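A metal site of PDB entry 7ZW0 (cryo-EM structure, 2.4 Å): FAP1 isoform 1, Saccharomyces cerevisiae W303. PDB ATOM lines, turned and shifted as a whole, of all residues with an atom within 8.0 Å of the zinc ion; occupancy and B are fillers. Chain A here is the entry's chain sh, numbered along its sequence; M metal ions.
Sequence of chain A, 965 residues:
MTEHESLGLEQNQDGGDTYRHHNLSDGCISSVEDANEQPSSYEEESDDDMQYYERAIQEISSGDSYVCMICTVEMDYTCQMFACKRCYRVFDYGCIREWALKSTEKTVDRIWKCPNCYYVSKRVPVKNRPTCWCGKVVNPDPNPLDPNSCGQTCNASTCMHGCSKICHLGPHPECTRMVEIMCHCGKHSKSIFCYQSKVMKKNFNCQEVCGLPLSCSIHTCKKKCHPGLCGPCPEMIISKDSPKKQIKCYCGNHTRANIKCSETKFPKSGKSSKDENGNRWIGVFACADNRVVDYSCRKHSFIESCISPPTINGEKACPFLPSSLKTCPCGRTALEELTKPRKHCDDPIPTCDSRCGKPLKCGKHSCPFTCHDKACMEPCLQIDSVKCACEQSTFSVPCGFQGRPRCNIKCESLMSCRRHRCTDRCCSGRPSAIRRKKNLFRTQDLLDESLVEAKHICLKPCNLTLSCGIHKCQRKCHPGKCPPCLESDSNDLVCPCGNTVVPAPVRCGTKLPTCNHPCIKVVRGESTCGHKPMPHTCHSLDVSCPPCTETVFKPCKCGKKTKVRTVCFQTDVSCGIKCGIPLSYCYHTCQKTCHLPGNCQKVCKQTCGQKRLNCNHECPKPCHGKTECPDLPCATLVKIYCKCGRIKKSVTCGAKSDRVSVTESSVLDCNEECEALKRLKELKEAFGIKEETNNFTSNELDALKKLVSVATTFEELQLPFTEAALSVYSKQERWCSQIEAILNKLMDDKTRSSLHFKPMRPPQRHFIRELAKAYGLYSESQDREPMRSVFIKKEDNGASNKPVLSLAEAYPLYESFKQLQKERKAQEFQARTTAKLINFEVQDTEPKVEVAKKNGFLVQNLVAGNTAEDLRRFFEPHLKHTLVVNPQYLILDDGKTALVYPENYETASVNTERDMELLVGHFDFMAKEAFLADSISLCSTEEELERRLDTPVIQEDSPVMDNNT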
ATOM      1  N   MET A  69     -17.614  -2.212  -6.997  1.00  0.00           N
ATOM      2  CA  MET A  69     -16.292  -1.585  -7.033  1.00  0.00           C
ATOM      3  C   MET A  69     -16.244  -0.077  -7.228  1.00  0.00           C
ATOM      4  O   MET A  69     -15.472   0.603  -6.555  1.00  0.00           O
ATOM      5  CB  MET A  69     -15.418  -2.275  -8.081  1.00  0.00           C
ATOM      6  CG  MET A  69     -15.140  -3.732  -7.767  1.00  0.00           C
ATOM      7  SD  MET A  69     -13.967  -4.511  -8.899  1.00  0.00           S
ATOM      8  CE  MET A  69     -12.496  -3.544  -8.578  1.00  0.00           C
ATOM      9  N   PHE A  82     -23.717  -6.026 -12.603  1.00  0.00           N
ATOM     10  CA  PHE A  82     -23.144  -6.172 -13.950  1.00  0.00           C
ATOM     11  C   PHE A  82     -21.997  -7.187 -13.942  1.00  0.00           C
ATOM     12  O   PHE A  82     -21.152  -7.146 -13.045  1.00  0.00           O
ATOM     13  CB  PHE A  82     -22.630  -4.845 -14.464  1.00  0.00           C
ATOM     14  CG  PHE A  82     -21.964  -4.939 -15.810  1.00  0.00           C
ATOM     15  CD1 PHE A  82     -22.725  -5.057 -16.956  1.00  0.00           C
ATOM     16  CD2 PHE A  82     -20.590  -4.898 -15.924  1.00  0.00           C
ATOM     17  CE1 PHE A  82     -22.124  -5.148 -18.203  1.00  0.00           C
ATOM     18  CE2 PHE A  82     -19.977  -4.997 -17.154  1.00  0.00           C
ATOM     19  CZ  PHE A  82     -20.744  -5.111 -18.293  1.00  0.00           C
ATOM     20  N   ALA A  83     -21.971  -8.091 -14.907  1.00  0.00           N
ATOM     21  CA  ALA A  83     -20.946  -9.128 -14.928  1.00  0.00           C
ATOM     22  C   ALA A  83     -20.052  -9.035 -16.145  1.00  0.00           C
ATOM     23  O   ALA A  83     -20.526  -8.817 -17.260  1.00  0.00           O
ATOM     24  CB  ALA A  83     -21.579 -10.498 -14.829  1.00  0.00           C
ATOM     25  N   CYS A  84     -18.756  -9.212 -15.946  1.00  0.00           N
ATOM     26  CA  CYS A  84     -17.825  -9.206 -17.067  1.00  0.00           C
ATOM     27  C   CYS A  84     -17.188 -10.572 -17.144  1.00  0.00           C
ATOM     28  O   CYS A  84     -16.746 -11.093 -16.131  1.00  0.00           O
ATOM     29  CB  CYS A  84     -16.750  -8.133 -16.897  1.00  0.00           C
ATOM     30  SG  CYS A  84     -15.425  -8.213 -18.115  1.00  0.00           S
ATOM     31  N   LYS A  85     -17.134 -11.162 -18.327  1.00  0.00           N
ATOM     32  CA  LYS A  85     -16.610 -12.512 -18.445  1.00  0.00           C
ATOM     33  C   LYS A  85     -15.152 -12.592 -18.042  1.00  0.00           C
ATOM     34  O   LYS A  85     -14.735 -13.542 -17.398  1.00  0.00           O
ATOM     35  CB  LYS A  85     -16.786 -13.037 -19.882  1.00  0.00           C
ATOM     36  CG  LYS A  85     -18.200 -13.509 -20.224  1.00  0.00           C
ATOM     37  CD  LYS A  85     -19.129 -12.356 -20.589  1.00  0.00           C
ATOM     38  CE  LYS A  85     -20.155 -12.102 -19.508  1.00  0.00           C
ATOM     39  NZ  LYS A  85     -20.842 -10.796 -19.698  1.00  0.00           N
ATOM     40  N   ARG A  86     -14.369 -11.587 -18.408  1.00  0.00           N
ATOM     41  CA  ARG A  86     -12.945 -11.629 -18.117  1.00  0.00           C
ATOM     42  C   ARG A  86     -12.649 -11.650 -16.612  1.00  0.00           C
ATOM     43  O   ARG A  86     -11.801 -12.423 -16.159  1.00  0.00           O
ATOM     44  CB  ARG A  86     -12.228 -10.457 -18.800  1.00  0.00           C
ATOM     45  CG  ARG A  86     -10.722 -10.643 -18.915  1.00  0.00           C
ATOM     46  CD  ARG A  86     -10.383 -11.841 -19.780  1.00  0.00           C
ATOM     47  NE  ARG A  86      -9.010 -12.295 -19.580  1.00  0.00           N
ATOM     48  CZ  ARG A  86      -8.650 -13.238 -18.713  1.00  0.00           C
ATOM     49  NH1 ARG A  86      -9.567 -13.835 -17.969  1.00  0.00           N
ATOM     50  NH2 ARG A  86      -7.374 -13.584 -18.590  1.00  0.00           N
ATOM     51  N   CYS A  87     -13.351 -10.831 -15.841  1.00  0.00           N
ATOM     52  CA  CYS A  87     -13.123 -10.801 -14.398  1.00  0.00           C
ATOM     53  C   CYS A  87     -14.124 -11.592 -13.584  1.00  0.00           C
ATOM     54  O   CYS A  87     -13.899 -11.811 -12.393  1.00  0.00           O
ATOM     55  CB  CYS A  87     -13.146  -9.363 -13.897  1.00  0.00           C
ATOM     56  SG  CYS A  87     -14.789  -8.615 -13.919  1.00  0.00           S
ATOM     57  N   TYR A  88     -15.198 -12.051 -14.205  1.00  0.00           N
ATOM     58  CA  TYR A  88     -16.266 -12.732 -13.470  1.00  0.00           C
ATOM     59  C   TYR A  88     -16.531 -12.109 -12.105  1.00  0.00           C
ATOM     60  O   TYR A  88     -16.638 -12.816 -11.097  1.00  0.00           O
ATOM     61  CB  TYR A  88     -16.022 -14.239 -13.384  1.00  0.00           C
ATOM     62  CG  TYR A  88     -16.458 -14.955 -14.637  1.00  0.00           C
ATOM     63  CD1 TYR A  88     -17.730 -14.742 -15.157  1.00  0.00           C
ATOM     64  CD2 TYR A  88     -15.619 -15.837 -15.288  1.00  0.00           C
ATOM     65  CE1 TYR A  88     -18.141 -15.389 -16.307  1.00  0.00           C
ATOM     66  CE2 TYR A  88     -16.017 -16.487 -16.438  1.00  0.00           C
ATOM     67  CZ  TYR A  88     -17.283 -16.252 -16.950  1.00  0.00           C
ATOM     68  OH  TYR A  88     -17.687 -16.898 -18.093  1.00  0.00           O
ATOM     69  N   ARG A  89     -16.654 -10.786 -12.066  1.00  0.00           N
ATOM     70  CA  ARG A  89     -16.914 -10.084 -10.827  1.00  0.00           C
ATOM     71  C   ARG A  89     -18.136  -9.200 -11.043  1.00  0.00           C
ATOM     72  O   ARG A  89     -18.442  -8.838 -12.182  1.00  0.00           O
ATOM     73  CB  ARG A  89     -15.676  -9.265 -10.440  1.00  0.00           C
ATOM     74  CG  ARG A  89     -15.889  -8.087  -9.505  1.00  0.00           C
ATOM     75  CD  ARG A  89     -15.447  -8.398  -8.088  1.00  0.00           C
ATOM     76  NE  ARG A  89     -15.778  -7.314  -7.169  1.00  0.00           N
ATOM     77  CZ  ARG A  89     -15.433  -7.285  -5.880  1.00  0.00           C
ATOM     78  NH1 ARG A  89     -14.728  -8.283  -5.367  1.00  0.00           N
ATOM     79  NH2 ARG A  89     -15.793  -6.263  -5.118  1.00  0.00           N
ATOM     80  N   VAL A  90     -18.846  -8.849  -9.982  1.00  0.00           N
ATOM     81  CA  VAL A  90     -20.060  -8.049 -10.115  1.00  0.00           C
ATOM     82  C   VAL A  90     -20.021  -6.681  -9.444  1.00  0.00           C
ATOM     83  O   VAL A  90     -19.509  -6.542  -8.324  1.00  0.00           O
ATOM     84  CB  VAL A  90     -21.289  -8.854  -9.673  1.00  0.00           C
ATOM     85  CG1 VAL A  90     -22.391  -7.974  -9.137  1.00  0.00           C
ATOM     86  CG2 VAL A  90     -21.786  -9.695 -10.827  1.00  0.00           C
ATOM     87  N   PHE A  91     -20.506  -5.653 -10.135  1.00  0.00           N
ATOM     88  CA  PHE A  91     -20.546  -4.309  -9.569  1.00  0.00           C
ATOM     89  C   PHE A  91     -21.972  -3.834  -9.742  1.00  0.00           C
ATOM     90  O   PHE A  91     -22.746  -4.467 -10.442  1.00  0.00           O
ATOM     91  CB  PHE A  91     -19.605  -3.381 -10.337  1.00  0.00           C
ATOM     92  CG  PHE A  91     -18.615  -4.097 -11.201  1.00  0.00           C
ATOM     93  CD1 PHE A  91     -18.947  -4.456 -12.505  1.00  0.00           C
ATOM     94  CD2 PHE A  91     -17.355  -4.416 -10.723  1.00  0.00           C
ATOM     95  CE1 PHE A  91     -18.032  -5.123 -13.305  1.00  0.00           C
ATOM     96  CE2 PHE A  91     -16.444  -5.070 -11.518  1.00  0.00           C
ATOM     97  CZ  PHE A  91     -16.785  -5.434 -12.813  1.00  0.00           C
ATOM     98  N   ILE A  96     -21.207   0.959 -12.535  1.00  0.00           N
ATOM     99  CA  ILE A  96     -20.246   0.589 -13.556  1.00  0.00           C
ATOM    100  C   ILE A  96     -20.514   1.341 -14.869  1.00  0.00           C
ATOM    101  O   ILE A  96     -19.578   1.608 -15.622  1.00  0.00           O
ATOM    102  CB  ILE A  96     -20.196  -0.941 -13.774  1.00  0.00           C
ATOM    103  CG1 ILE A  96     -18.863  -1.359 -14.401  1.00  0.00           C
ATOM    104  CG2 ILE A  96     -21.342  -1.429 -14.654  1.00  0.00           C
ATOM    105  CD1 ILE A  96     -17.662  -1.031 -13.545  1.00  0.00           C
ATOM    106  N   TRP A 112     -14.852   1.526 -23.032  1.00  0.00           N
ATOM    107  CA  TRP A 112     -15.062   1.373 -21.594  1.00  0.00           C
ATOM    108  C   TRP A 112     -14.122   0.326 -20.980  1.00  0.00           C
ATOM    109  O   TRP A 112     -13.761  -0.633 -21.642  1.00  0.00           O
ATOM    110  CB  TRP A 112     -16.526   1.029 -21.314  1.00  0.00           C
ATOM    111  CG  TRP A 112     -16.789  -0.407 -21.021  1.00  0.00           C
ATOM    112  CD1 TRP A 112     -16.970  -1.411 -21.921  1.00  0.00           C
ATOM    113  CD2 TRP A 112     -16.914  -1.009 -19.717  1.00  0.00           C
ATOM    114  NE1 TRP A 112     -17.201  -2.593 -21.262  1.00  0.00           N
ATOM    115  CE2 TRP A 112     -17.165  -2.372 -19.912  1.00  0.00           C
ATOM    116  CE3 TRP A 112     -16.832  -0.513 -18.413  1.00  0.00           C
ATOM    117  CZ2 TRP A 112     -17.337  -3.253 -18.856  1.00  0.00           C
ATOM    118  CZ3 TRP A 112     -17.002  -1.389 -17.374  1.00  0.00           C
ATOM    119  CH2 TRP A 112     -17.251  -2.746 -17.585  1.00  0.00           C
ATOM    120  N   LYS A 113     -13.734   0.498 -19.714  1.00  0.00           N
ATOM    121  CA  LYS A 113     -12.767  -0.438 -19.104  1.00  0.00           C
ATOM    122  C   LYS A 113     -13.317  -1.138 -17.869  1.00  0.00           C
ATOM    123  O   LYS A 113     -13.965  -0.510 -17.047  1.00  0.00           O
ATOM    124  CB  LYS A 113     -11.475   0.306 -18.744  1.00  0.00           C
ATOM    125  CG  LYS A 113     -10.327  -0.611 -18.343  1.00  0.00           C
ATOM    126  CD  LYS A 113      -8.997   0.106 -18.464  1.00  0.00           C
ATOM    127  CE  LYS A 113      -7.854  -0.892 -18.439  1.00  0.00           C
ATOM    128  NZ  LYS A 113      -6.545  -0.232 -18.726  1.00  0.00           N
ATOM    129  N   CYS A 114     -13.053  -2.422 -17.737  1.00  0.00           N
ATOM    130  CA  CYS A 114     -13.492  -3.146 -16.561  1.00  0.00           C
ATOM    131  C   CYS A 114     -12.370  -3.191 -15.548  1.00  0.00           C
ATOM    132  O   CYS A 114     -11.310  -3.736 -15.832  1.00  0.00           O
ATOM    133  CB  CYS A 114     -13.923  -4.559 -16.928  1.00  0.00           C
ATOM    134  SG  CYS A 114     -14.541  -5.501 -15.522  1.00  0.00           S
ATOM    135  N   PRO A 115     -12.588  -2.641 -14.350  1.00  0.00           N
ATOM    136  CA  PRO A 115     -11.518  -2.547 -13.344  1.00  0.00           C
ATOM    137  C   PRO A 115     -10.954  -3.846 -12.771  1.00  0.00           C
ATOM    138  O   PRO A 115      -9.737  -3.928 -12.609  1.00  0.00           O
ATOM    139  CB  PRO A 115     -12.173  -1.764 -12.197  1.00  0.00           C
ATOM    140  CG  PRO A 115     -13.387  -1.117 -12.795  1.00  0.00           C
ATOM    141  CD  PRO A 115     -13.848  -2.050 -13.866  1.00  0.00           C
ATOM    142  N   ASN A 116     -11.789  -4.824 -12.468  1.00  0.00           N
ATOM    143  CA  ASN A 116     -11.275  -6.032 -11.815  1.00  0.00           C
ATOM    144  C   ASN A 116     -10.288  -6.789 -12.675  1.00  0.00           C
ATOM    145  O   ASN A 116      -9.253  -7.252 -12.184  1.00  0.00           O
ATOM    146  CB  ASN A 116     -12.423  -6.947 -11.384  1.00  0.00           C
ATOM    147  CG  ASN A 116     -11.995  -7.939 -10.308  1.00  0.00           C
ATOM    148  OD1 ASN A 116     -11.456  -7.542  -9.272  1.00  0.00           O
ATOM    149  ND2 ASN A 116     -12.254  -9.215 -10.541  1.00  0.00           N
ATOM    150  N   CYS A 117     -10.577  -6.916 -13.961  1.00  0.00           N
ATOM    151  CA  CYS A 117      -9.643  -7.567 -14.869  1.00  0.00           C
ATOM    152  C   CYS A 117      -8.758  -6.537 -15.522  1.00  0.00           C
ATOM    153  O   CYS A 117      -7.904  -6.893 -16.341  1.00  0.00           O
ATOM    154  CB  CYS A 117     -10.391  -8.361 -15.931  1.00  0.00           C
ATOM    155  SG  CYS A 117     -11.803  -7.488 -16.618  1.00  0.00           S
ATOM    156  N   TYR A 118      -8.960  -5.266 -15.189  1.00  0.00           N
ATOM    157  CA  TYR A 118      -8.201  -4.184 -15.812  1.00  0.00           C
ATOM    158  C   TYR A 118      -8.239  -4.417 -17.306  1.00  0.00           C
ATOM    159  O   TYR A 118      -7.217  -4.331 -17.983  1.00  0.00           O
ATOM    160  CB  TYR A 118      -6.758  -4.146 -15.280  1.00  0.00           C
ATOM    161  CG  TYR A 118      -6.095  -2.803 -15.411  1.00  0.00           C
ATOM    162  CD1 TYR A 118      -6.626  -1.675 -14.793  1.00  0.00           C
ATOM    163  CD2 TYR A 118      -4.926  -2.653 -16.146  1.00  0.00           C
ATOM    164  CE1 TYR A 118      -6.021  -0.445 -14.917  1.00  0.00           C
ATOM    165  CE2 TYR A 118      -4.307  -1.426 -16.270  1.00  0.00           C
ATOM    166  CZ  TYR A 118      -4.858  -0.323 -15.644  1.00  0.00           C
ATOM    167  OH  TYR A 118      -4.246   0.907 -15.761  1.00  0.00           O
ATOM    168  N   TYR A 119      -9.421  -4.723 -17.830  1.00  0.00           N
ATOM    169  CA  TYR A 119      -9.539  -5.041 -19.249  1.00  0.00           C
ATOM    170  C   TYR A 119     -10.502  -4.119 -19.937  1.00  0.00           C
ATOM    171  O   TYR A 119     -11.634  -3.946 -19.489  1.00  0.00           O
ATOM    172  CB  TYR A 119      -9.928  -6.519 -19.408  1.00  0.00           C
ATOM    173  CG  TYR A 119     -10.990  -6.850 -20.442  1.00  0.00           C
ATOM    174  CD1 TYR A 119     -12.336  -6.864 -20.110  1.00  0.00           C
ATOM    175  CD2 TYR A 119     -10.637  -7.205 -21.736  1.00  0.00           C
ATOM    176  CE1 TYR A 119     -13.306  -7.174 -21.038  1.00  0.00           C
ATOM    177  CE2 TYR A 119     -11.601  -7.519 -22.671  1.00  0.00           C
ATOM    178  CZ  TYR A 119     -12.924  -7.501 -22.320  1.00  0.00           C
ATOM    179  OH  TYR A 119     -13.894  -7.811 -23.248  1.00  0.00           O
ATOM    180  N   VAL A 120     -10.057  -3.484 -21.014  1.00  0.00           N
ATOM    181  CA  VAL A 120     -10.944  -2.611 -21.766  1.00  0.00           C
ATOM    182  C   VAL A 120     -11.870  -3.414 -22.651  1.00  0.00           C
ATOM    183  O   VAL A 120     -11.482  -4.440 -23.192  1.00  0.00           O
ATOM    184  CB  VAL A 120     -10.139  -1.639 -22.640  1.00  0.00           C
ATOM    185  CG1 VAL A 120     -10.473  -0.196 -22.274  1.00  0.00           C
ATOM    186  CG2 VAL A 120      -8.658  -1.894 -22.476  1.00  0.00           C
ATOM    187  N   SER A 121     -13.093  -2.945 -22.820  1.00  0.00           N
ATOM    188  CA  SER A 121     -14.041  -3.606 -23.715  1.00  0.00           C
ATOM    189  C   SER A 121     -14.632  -2.536 -24.603  1.00  0.00           C
ATOM    190  O   SER A 121     -14.482  -1.344 -24.309  1.00  0.00           O
ATOM    191  CB  SER A 121     -15.104  -4.382 -22.939  1.00  0.00           C
ATOM    192  OG  SER A 121     -15.958  -5.103 -23.815  1.00  0.00           O
HETATM  193 ZN    ZN M   1     -14.319  -7.488 -15.966  1.00  0.00          ZN
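The side-chain sulfur (SG) of Cys 84 lies close to the backbone NH (N) of Arg 86. The backbone NH (N) of Arg 89 sits close to the side-chain sulfur (SG) of Cys 87 (3.4 Å). N of Cys 114 is in hydrogen-bond range of O of Tyr 119 (2.7 Å).
Within 4 Å of the zinc ion: Cys 84, Cys 87, Cys 114 and Cys 117. The nearest printed residue that does not touch the zinc ion is Phe 91 (4.5 Å).
The zinc ion is bound by the side-chain sulfur of Cys 114, the side-chain sulfur of Cys 87, the side-chain sulfur of Cys 84 and the side-chain sulfur of Cys 117.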
